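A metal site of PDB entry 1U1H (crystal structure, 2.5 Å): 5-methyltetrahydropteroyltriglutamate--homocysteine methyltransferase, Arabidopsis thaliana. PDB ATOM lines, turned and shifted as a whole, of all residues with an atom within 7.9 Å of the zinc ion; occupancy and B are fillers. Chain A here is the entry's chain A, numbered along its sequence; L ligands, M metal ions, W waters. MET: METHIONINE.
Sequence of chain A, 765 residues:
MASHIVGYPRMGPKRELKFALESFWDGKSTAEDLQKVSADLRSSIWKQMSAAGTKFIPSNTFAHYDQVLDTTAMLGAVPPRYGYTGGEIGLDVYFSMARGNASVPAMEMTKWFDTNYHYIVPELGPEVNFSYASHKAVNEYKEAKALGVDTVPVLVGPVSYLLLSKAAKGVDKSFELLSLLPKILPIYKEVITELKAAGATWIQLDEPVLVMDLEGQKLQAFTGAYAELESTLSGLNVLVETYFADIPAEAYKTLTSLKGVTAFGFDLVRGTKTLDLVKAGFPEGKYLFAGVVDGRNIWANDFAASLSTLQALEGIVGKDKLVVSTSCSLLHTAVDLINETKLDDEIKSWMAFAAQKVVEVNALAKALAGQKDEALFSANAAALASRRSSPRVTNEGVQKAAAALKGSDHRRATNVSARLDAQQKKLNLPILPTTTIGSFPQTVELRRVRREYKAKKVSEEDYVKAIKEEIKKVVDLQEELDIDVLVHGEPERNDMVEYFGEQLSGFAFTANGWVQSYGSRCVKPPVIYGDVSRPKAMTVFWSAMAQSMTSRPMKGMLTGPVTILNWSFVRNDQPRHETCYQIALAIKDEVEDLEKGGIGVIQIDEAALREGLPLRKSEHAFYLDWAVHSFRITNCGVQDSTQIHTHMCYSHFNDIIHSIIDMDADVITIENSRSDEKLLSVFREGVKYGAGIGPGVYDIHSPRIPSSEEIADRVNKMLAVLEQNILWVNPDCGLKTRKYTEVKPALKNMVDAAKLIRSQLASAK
The side-chain sulfur of Cys 649 lies close to a sulfur (SD) of the ligand, 3.6 Å away.
O of Ile 437 is in hydrogen-bond range of N of the ligand, 3.1 Å away.
The side-chain carboxylate of Asp 605 is in salt-bridge range of a nitrogen (N) of the ligand (2.9 Å).
O of Thr 669 sits close to ND1 of His 647 (3.2 Å).
O of His 647 sits at hydrogen-bond distance from N of Glu 606, at 2.7 Å.
Within 4 Å of the zinc ion: His 647, Cys 649 and Cys 733.
The nearest printed residue that does not touch the zinc ion is Asp 732 (4.1 Å).
NE2 of His 647 binds the zinc ion.
The zinc ion is bound by water W1 (2.3 Å).
SG of Cys 649 is bound to the zinc ion (2.4 Å).
SG of Cys 733 is bound to the zinc ion (2.4 Å).
The zinc ion has four donor atoms within binding distance.
Water W1 bridges the backbone carbonyl oxygen (O) of Asp 732 (2.7 Å) and the side-chain carboxylate (OE2) of Glu 671 (2.8 Å).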
ATOM      1  N   ILE A 437      10.861   2.466 -24.301  1.00  0.00           N
ATOM      2  CA  ILE A 437      11.864   3.249 -25.001  1.00  0.00           C
ATOM      3  C   ILE A 437      11.912   3.144 -26.527  1.00  0.00           C
ATOM      4  O   ILE A 437      12.531   3.982 -27.176  1.00  0.00           O
ATOM      5  CB  ILE A 437      13.243   2.961 -24.436  1.00  0.00           C
ATOM      6  CG1 ILE A 437      13.209   3.130 -22.917  1.00  0.00           C
ATOM      7  CG2 ILE A 437      14.275   3.908 -25.033  1.00  0.00           C
ATOM      8  CD1 ILE A 437      12.649   4.458 -22.462  1.00  0.00           C
ATOM      9  N   MET A 496      19.994   1.967 -35.409  1.00  0.00           N
ATOM     10  CA  MET A 496      19.643   3.325 -34.970  1.00  0.00           C
ATOM     11  C   MET A 496      20.103   4.406 -35.919  1.00  0.00           C
ATOM     12  O   MET A 496      19.344   5.300 -36.286  1.00  0.00           O
ATOM     13  CB  MET A 496      20.305   3.639 -33.637  1.00  0.00           C
ATOM     14  CG  MET A 496      19.556   3.289 -32.400  1.00  0.00           C
ATOM     15  SD  MET A 496      20.685   3.910 -30.968  1.00  0.00           S
ATOM     16  CE  MET A 496      20.032   5.730 -30.763  1.00  0.00           C
ATOM     17  N   ASP A 605      16.164  10.037 -29.224  1.00  0.00           N
ATOM     18  CA  ASP A 605      17.154   9.471 -28.312  1.00  0.00           C
ATOM     19  C   ASP A 605      18.586   9.809 -28.696  1.00  0.00           C
ATOM     20  O   ASP A 605      18.997   9.670 -29.854  1.00  0.00           O
ATOM     21  CB  ASP A 605      16.966   7.949 -28.187  1.00  0.00           C
ATOM     22  CG  ASP A 605      16.772   7.260 -29.524  1.00  0.00           C
ATOM     23  OD1 ASP A 605      17.448   7.663 -30.489  1.00  0.00           O
ATOM     24  OD2 ASP A 605      15.957   6.307 -29.615  1.00  0.00           O
ATOM     25  N   GLU A 606      19.331  10.302 -27.711  1.00  0.00           N
ATOM     26  CA  GLU A 606      20.729  10.661 -27.886  1.00  0.00           C
ATOM     27  C   GLU A 606      21.520   9.654 -27.064  1.00  0.00           C
ATOM     28  O   GLU A 606      22.093   9.975 -26.029  1.00  0.00           O
ATOM     29  CB  GLU A 606      20.984  12.080 -27.395  1.00  0.00           C
ATOM     30  CG  GLU A 606      20.544  13.147 -28.385  1.00  0.00           C
ATOM     31  CD  GLU A 606      21.451  13.189 -29.599  1.00  0.00           C
ATOM     32  OE1 GLU A 606      21.869  12.108 -30.067  1.00  0.00           O
ATOM     33  OE2 GLU A 606      21.738  14.284 -30.097  1.00  0.00           O
ATOM     34  N   ALA A 607      21.526   8.423 -27.560  1.00  0.00           N
ATOM     35  CA  ALA A 607      22.202   7.312 -26.919  1.00  0.00           C
ATOM     36  C   ALA A 607      23.672   7.584 -26.681  1.00  0.00           C
ATOM     37  O   ALA A 607      24.260   7.063 -25.737  1.00  0.00           O
ATOM     38  CB  ALA A 607      22.055   6.052 -27.780  1.00  0.00           C
ATOM     39  N   HIS A 647      15.838  10.297 -25.042  1.00  0.00           N
ATOM     40  CA  HIS A 647      16.334   9.135 -24.316  1.00  0.00           C
ATOM     41  C   HIS A 647      17.871   9.115 -24.283  1.00  0.00           C
ATOM     42  O   HIS A 647      18.513   9.380 -25.297  1.00  0.00           O
ATOM     43  CB  HIS A 647      15.811   7.857 -24.957  1.00  0.00           C
ATOM     44  CG  HIS A 647      16.410   6.612 -24.378  1.00  0.00           C
ATOM     45  ND1 HIS A 647      16.280   6.275 -23.052  1.00  0.00           N
ATOM     46  CD2 HIS A 647      17.193   5.659 -24.938  1.00  0.00           C
ATOM     47  CE1 HIS A 647      16.944   5.158 -22.817  1.00  0.00           C
ATOM     48  NE2 HIS A 647      17.504   4.763 -23.942  1.00  0.00           N
ATOM     49  N   MET A 648      18.449   8.784 -23.132  1.00  0.00           N
ATOM     50  CA  MET A 648      19.913   8.738 -23.005  1.00  0.00           C
ATOM     51  C   MET A 648      20.436   7.546 -22.214  1.00  0.00           C
ATOM     52  O   MET A 648      20.191   7.415 -21.020  1.00  0.00           O
ATOM     53  CB  MET A 648      20.425  10.033 -22.373  1.00  0.00           C
ATOM     54  CG  MET A 648      20.146  11.259 -23.215  1.00  0.00           C
ATOM     55  SD  MET A 648      20.562  12.892 -22.302  1.00  0.00           S
ATOM     56  CE  MET A 648      19.028  12.944 -21.132  1.00  0.00           C
ATOM     57  N   CYS A 649      21.197   6.696 -22.895  1.00  0.00           N
ATOM     58  CA  CYS A 649      21.766   5.502 -22.284  1.00  0.00           C
ATOM     59  C   CYS A 649      22.853   5.786 -21.254  1.00  0.00           C
ATOM     60  O   CYS A 649      24.010   5.474 -21.487  1.00  0.00           O
ATOM     61  CB  CYS A 649      22.316   4.598 -23.377  1.00  0.00           C
ATOM     62  SG  CYS A 649      21.222   4.421 -24.797  1.00  0.00           S
ATOM     63  N   TYR A 650      22.479   6.356 -20.110  1.00  0.00           N
ATOM     64  CA  TYR A 650      23.443   6.672 -19.056  1.00  0.00           C
ATOM     65  C   TYR A 650      22.743   6.699 -17.687  1.00  0.00           C
ATOM     66  O   TYR A 650      21.533   6.850 -17.609  1.00  0.00           O
ATOM     67  CB  TYR A 650      24.071   8.051 -19.299  1.00  0.00           C
ATOM     68  CG  TYR A 650      24.805   8.193 -20.616  1.00  0.00           C
ATOM     69  CD1 TYR A 650      26.050   7.589 -20.822  1.00  0.00           C
ATOM     70  CD2 TYR A 650      24.262   8.945 -21.658  1.00  0.00           C
ATOM     71  CE1 TYR A 650      26.727   7.738 -22.025  1.00  0.00           C
ATOM     72  CE2 TYR A 650      24.934   9.107 -22.864  1.00  0.00           C
ATOM     73  CZ  TYR A 650      26.166   8.496 -23.043  1.00  0.00           C
ATOM     74  OH  TYR A 650      26.849   8.672 -24.237  1.00  0.00           O
ATOM     75  N   THR A 669      14.236  10.324 -20.451  1.00  0.00           N
ATOM     76  CA  THR A 669      14.291   9.006 -19.839  1.00  0.00           C
ATOM     77  C   THR A 669      15.756   8.575 -19.824  1.00  0.00           C
ATOM     78  O   THR A 669      16.434   8.619 -20.854  1.00  0.00           O
ATOM     79  CB  THR A 669      13.424   8.023 -20.645  1.00  0.00           C
ATOM     80  OG1 THR A 669      13.345   6.790 -19.930  1.00  0.00           O
ATOM     81  CG2 THR A 669      14.018   7.779 -22.002  1.00  0.00           C
ATOM     82  N   ILE A 670      16.242   8.185 -18.657  1.00  0.00           N
ATOM     83  CA  ILE A 670      17.632   7.772 -18.517  1.00  0.00           C
ATOM     84  C   ILE A 670      17.732   6.324 -18.001  1.00  0.00           C
ATOM     85  O   ILE A 670      16.716   5.657 -17.808  1.00  0.00           O
ATOM     86  CB  ILE A 670      18.385   8.683 -17.521  1.00  0.00           C
ATOM     87  CG1 ILE A 670      17.785   8.499 -16.119  1.00  0.00           C
ATOM     88  CG2 ILE A 670      18.293  10.144 -17.956  1.00  0.00           C
ATOM     89  CD1 ILE A 670      18.529   9.247 -15.022  1.00  0.00           C
ATOM     90  N   GLU A 671      18.957   5.866 -17.775  1.00  0.00           N
ATOM     91  CA  GLU A 671      19.218   4.521 -17.259  1.00  0.00           C
ATOM     92  C   GLU A 671      19.202   4.544 -15.738  1.00  0.00           C
ATOM     93  O   GLU A 671      19.788   5.433 -15.119  1.00  0.00           O
ATOM     94  CB  GLU A 671      20.564   4.020 -17.735  1.00  0.00           C
ATOM     95  CG  GLU A 671      20.502   3.263 -19.033  1.00  0.00           C
ATOM     96  CD  GLU A 671      21.859   2.807 -19.493  1.00  0.00           C
ATOM     97  OE1 GLU A 671      22.658   2.403 -18.625  1.00  0.00           O
ATOM     98  OE2 GLU A 671      22.107   2.827 -20.710  1.00  0.00           O
ATOM     99  N   ILE A 700      17.094  -4.100 -19.018  1.00  0.00           N
ATOM    100  CA  ILE A 700      16.894  -4.845 -20.255  1.00  0.00           C
ATOM    101  C   ILE A 700      18.083  -5.704 -20.686  1.00  0.00           C
ATOM    102  O   ILE A 700      18.011  -6.425 -21.680  1.00  0.00           O
ATOM    103  CB  ILE A 700      16.581  -3.907 -21.431  1.00  0.00           C
ATOM    104  CG1 ILE A 700      17.749  -2.941 -21.652  1.00  0.00           C
ATOM    105  CG2 ILE A 700      15.286  -3.151 -21.157  1.00  0.00           C
ATOM    106  CD1 ILE A 700      17.967  -2.571 -23.100  1.00  0.00           C
ATOM    107  N   HIS A 701      19.185  -5.623 -19.958  1.00  0.00           N
ATOM    108  CA  HIS A 701      20.359  -6.408 -20.311  1.00  0.00           C
ATOM    109  C   HIS A 701      20.396  -7.760 -19.621  1.00  0.00           C
ATOM    110  O   HIS A 701      21.243  -8.592 -19.921  1.00  0.00           O
ATOM    111  CB  HIS A 701      21.631  -5.608 -20.012  1.00  0.00           C
ATOM    112  CG  HIS A 701      21.814  -4.415 -20.896  1.00  0.00           C
ATOM    113  ND1 HIS A 701      21.894  -3.127 -20.408  1.00  0.00           N
ATOM    114  CD2 HIS A 701      21.933  -4.322 -22.233  1.00  0.00           C
ATOM    115  CE1 HIS A 701      22.049  -2.287 -21.416  1.00  0.00           C
ATOM    116  NE2 HIS A 701      22.076  -2.987 -22.536  1.00  0.00           N
ATOM    117  N   PRO A 731      11.170   1.218 -18.942  1.00  0.00           N
ATOM    118  CA  PRO A 731      12.376   0.382 -18.833  1.00  0.00           C
ATOM    119  C   PRO A 731      13.691   1.159 -18.930  1.00  0.00           C
ATOM    120  O   PRO A 731      13.693   2.379 -19.089  1.00  0.00           O
ATOM    121  CB  PRO A 731      12.219  -0.611 -19.983  1.00  0.00           C
ATOM    122  CG  PRO A 731      10.727  -0.620 -20.242  1.00  0.00           C
ATOM    123  CD  PRO A 731      10.379   0.836 -20.114  1.00  0.00           C
ATOM    124  N   ASP A 732      14.797   0.434 -18.851  1.00  0.00           N
ATOM    125  CA  ASP A 732      16.146   0.999 -18.925  1.00  0.00           C
ATOM    126  C   ASP A 732      16.510   1.428 -20.335  1.00  0.00           C
ATOM    127  O   ASP A 732      17.262   2.379 -20.531  1.00  0.00           O
ATOM    128  CB  ASP A 732      17.185  -0.029 -18.466  1.00  0.00           C
ATOM    129  CG  ASP A 732      17.676   0.213 -17.055  1.00  0.00           C
ATOM    130  OD1 ASP A 732      17.371   1.287 -16.491  1.00  0.00           O
ATOM    131  OD2 ASP A 732      18.391  -0.664 -16.519  1.00  0.00           O
ATOM    132  N   CYS A 733      15.993   0.694 -21.318  1.00  0.00           N
ATOM    133  CA  CYS A 733      16.253   0.982 -22.719  1.00  0.00           C
ATOM    134  C   CYS A 733      15.306   0.172 -23.586  1.00  0.00           C
ATOM    135  O   CYS A 733      14.284  -0.315 -23.098  1.00  0.00           O
ATOM    136  CB  CYS A 733      17.701   0.643 -23.077  1.00  0.00           C
ATOM    137  SG  CYS A 733      18.232   1.262 -24.710  1.00  0.00           S
ATOM    138  N   GLY A 734      15.646   0.035 -24.856  1.00  0.00           N
ATOM    139  CA  GLY A 734      14.821  -0.727 -25.794  1.00  0.00           C
ATOM    140  C   GLY A 734      14.711  -2.176 -25.373  1.00  0.00           C
ATOM    141  O   GLY A 734      15.345  -2.599 -24.402  1.00  0.00           O
HETATM  142  N   MET L   1      14.584   3.792 -29.427  1.00  0.00           N
HETATM  143  CA  MET L   1      15.601   2.738 -29.711  1.00  0.00           C
HETATM  144  C   MET L   1      15.286   1.471 -28.923  1.00  0.00           C
HETATM  145  O   MET L   1      14.301   1.466 -28.161  1.00  0.00           O
HETATM  146  CB  MET L   1      16.993   3.244 -29.341  1.00  0.00           C
HETATM  147  CG  MET L   1      17.253   3.340 -27.850  1.00  0.00           C
HETATM  148  SD  MET L   1      18.859   4.084 -27.468  1.00  0.00           S
HETATM  149  CE  MET L   1      20.007   2.720 -27.798  1.00  0.00           C
HETATM  150  OXT MET L   1      16.044   0.493 -29.087  1.00  0.00           O
HETATM  151 ZN    ZN M   1      19.197   3.384 -23.962  1.00  0.00          ZN
HETATM  152  O   HOH W   1      19.507   3.226 -21.691  1.00  0.00           O
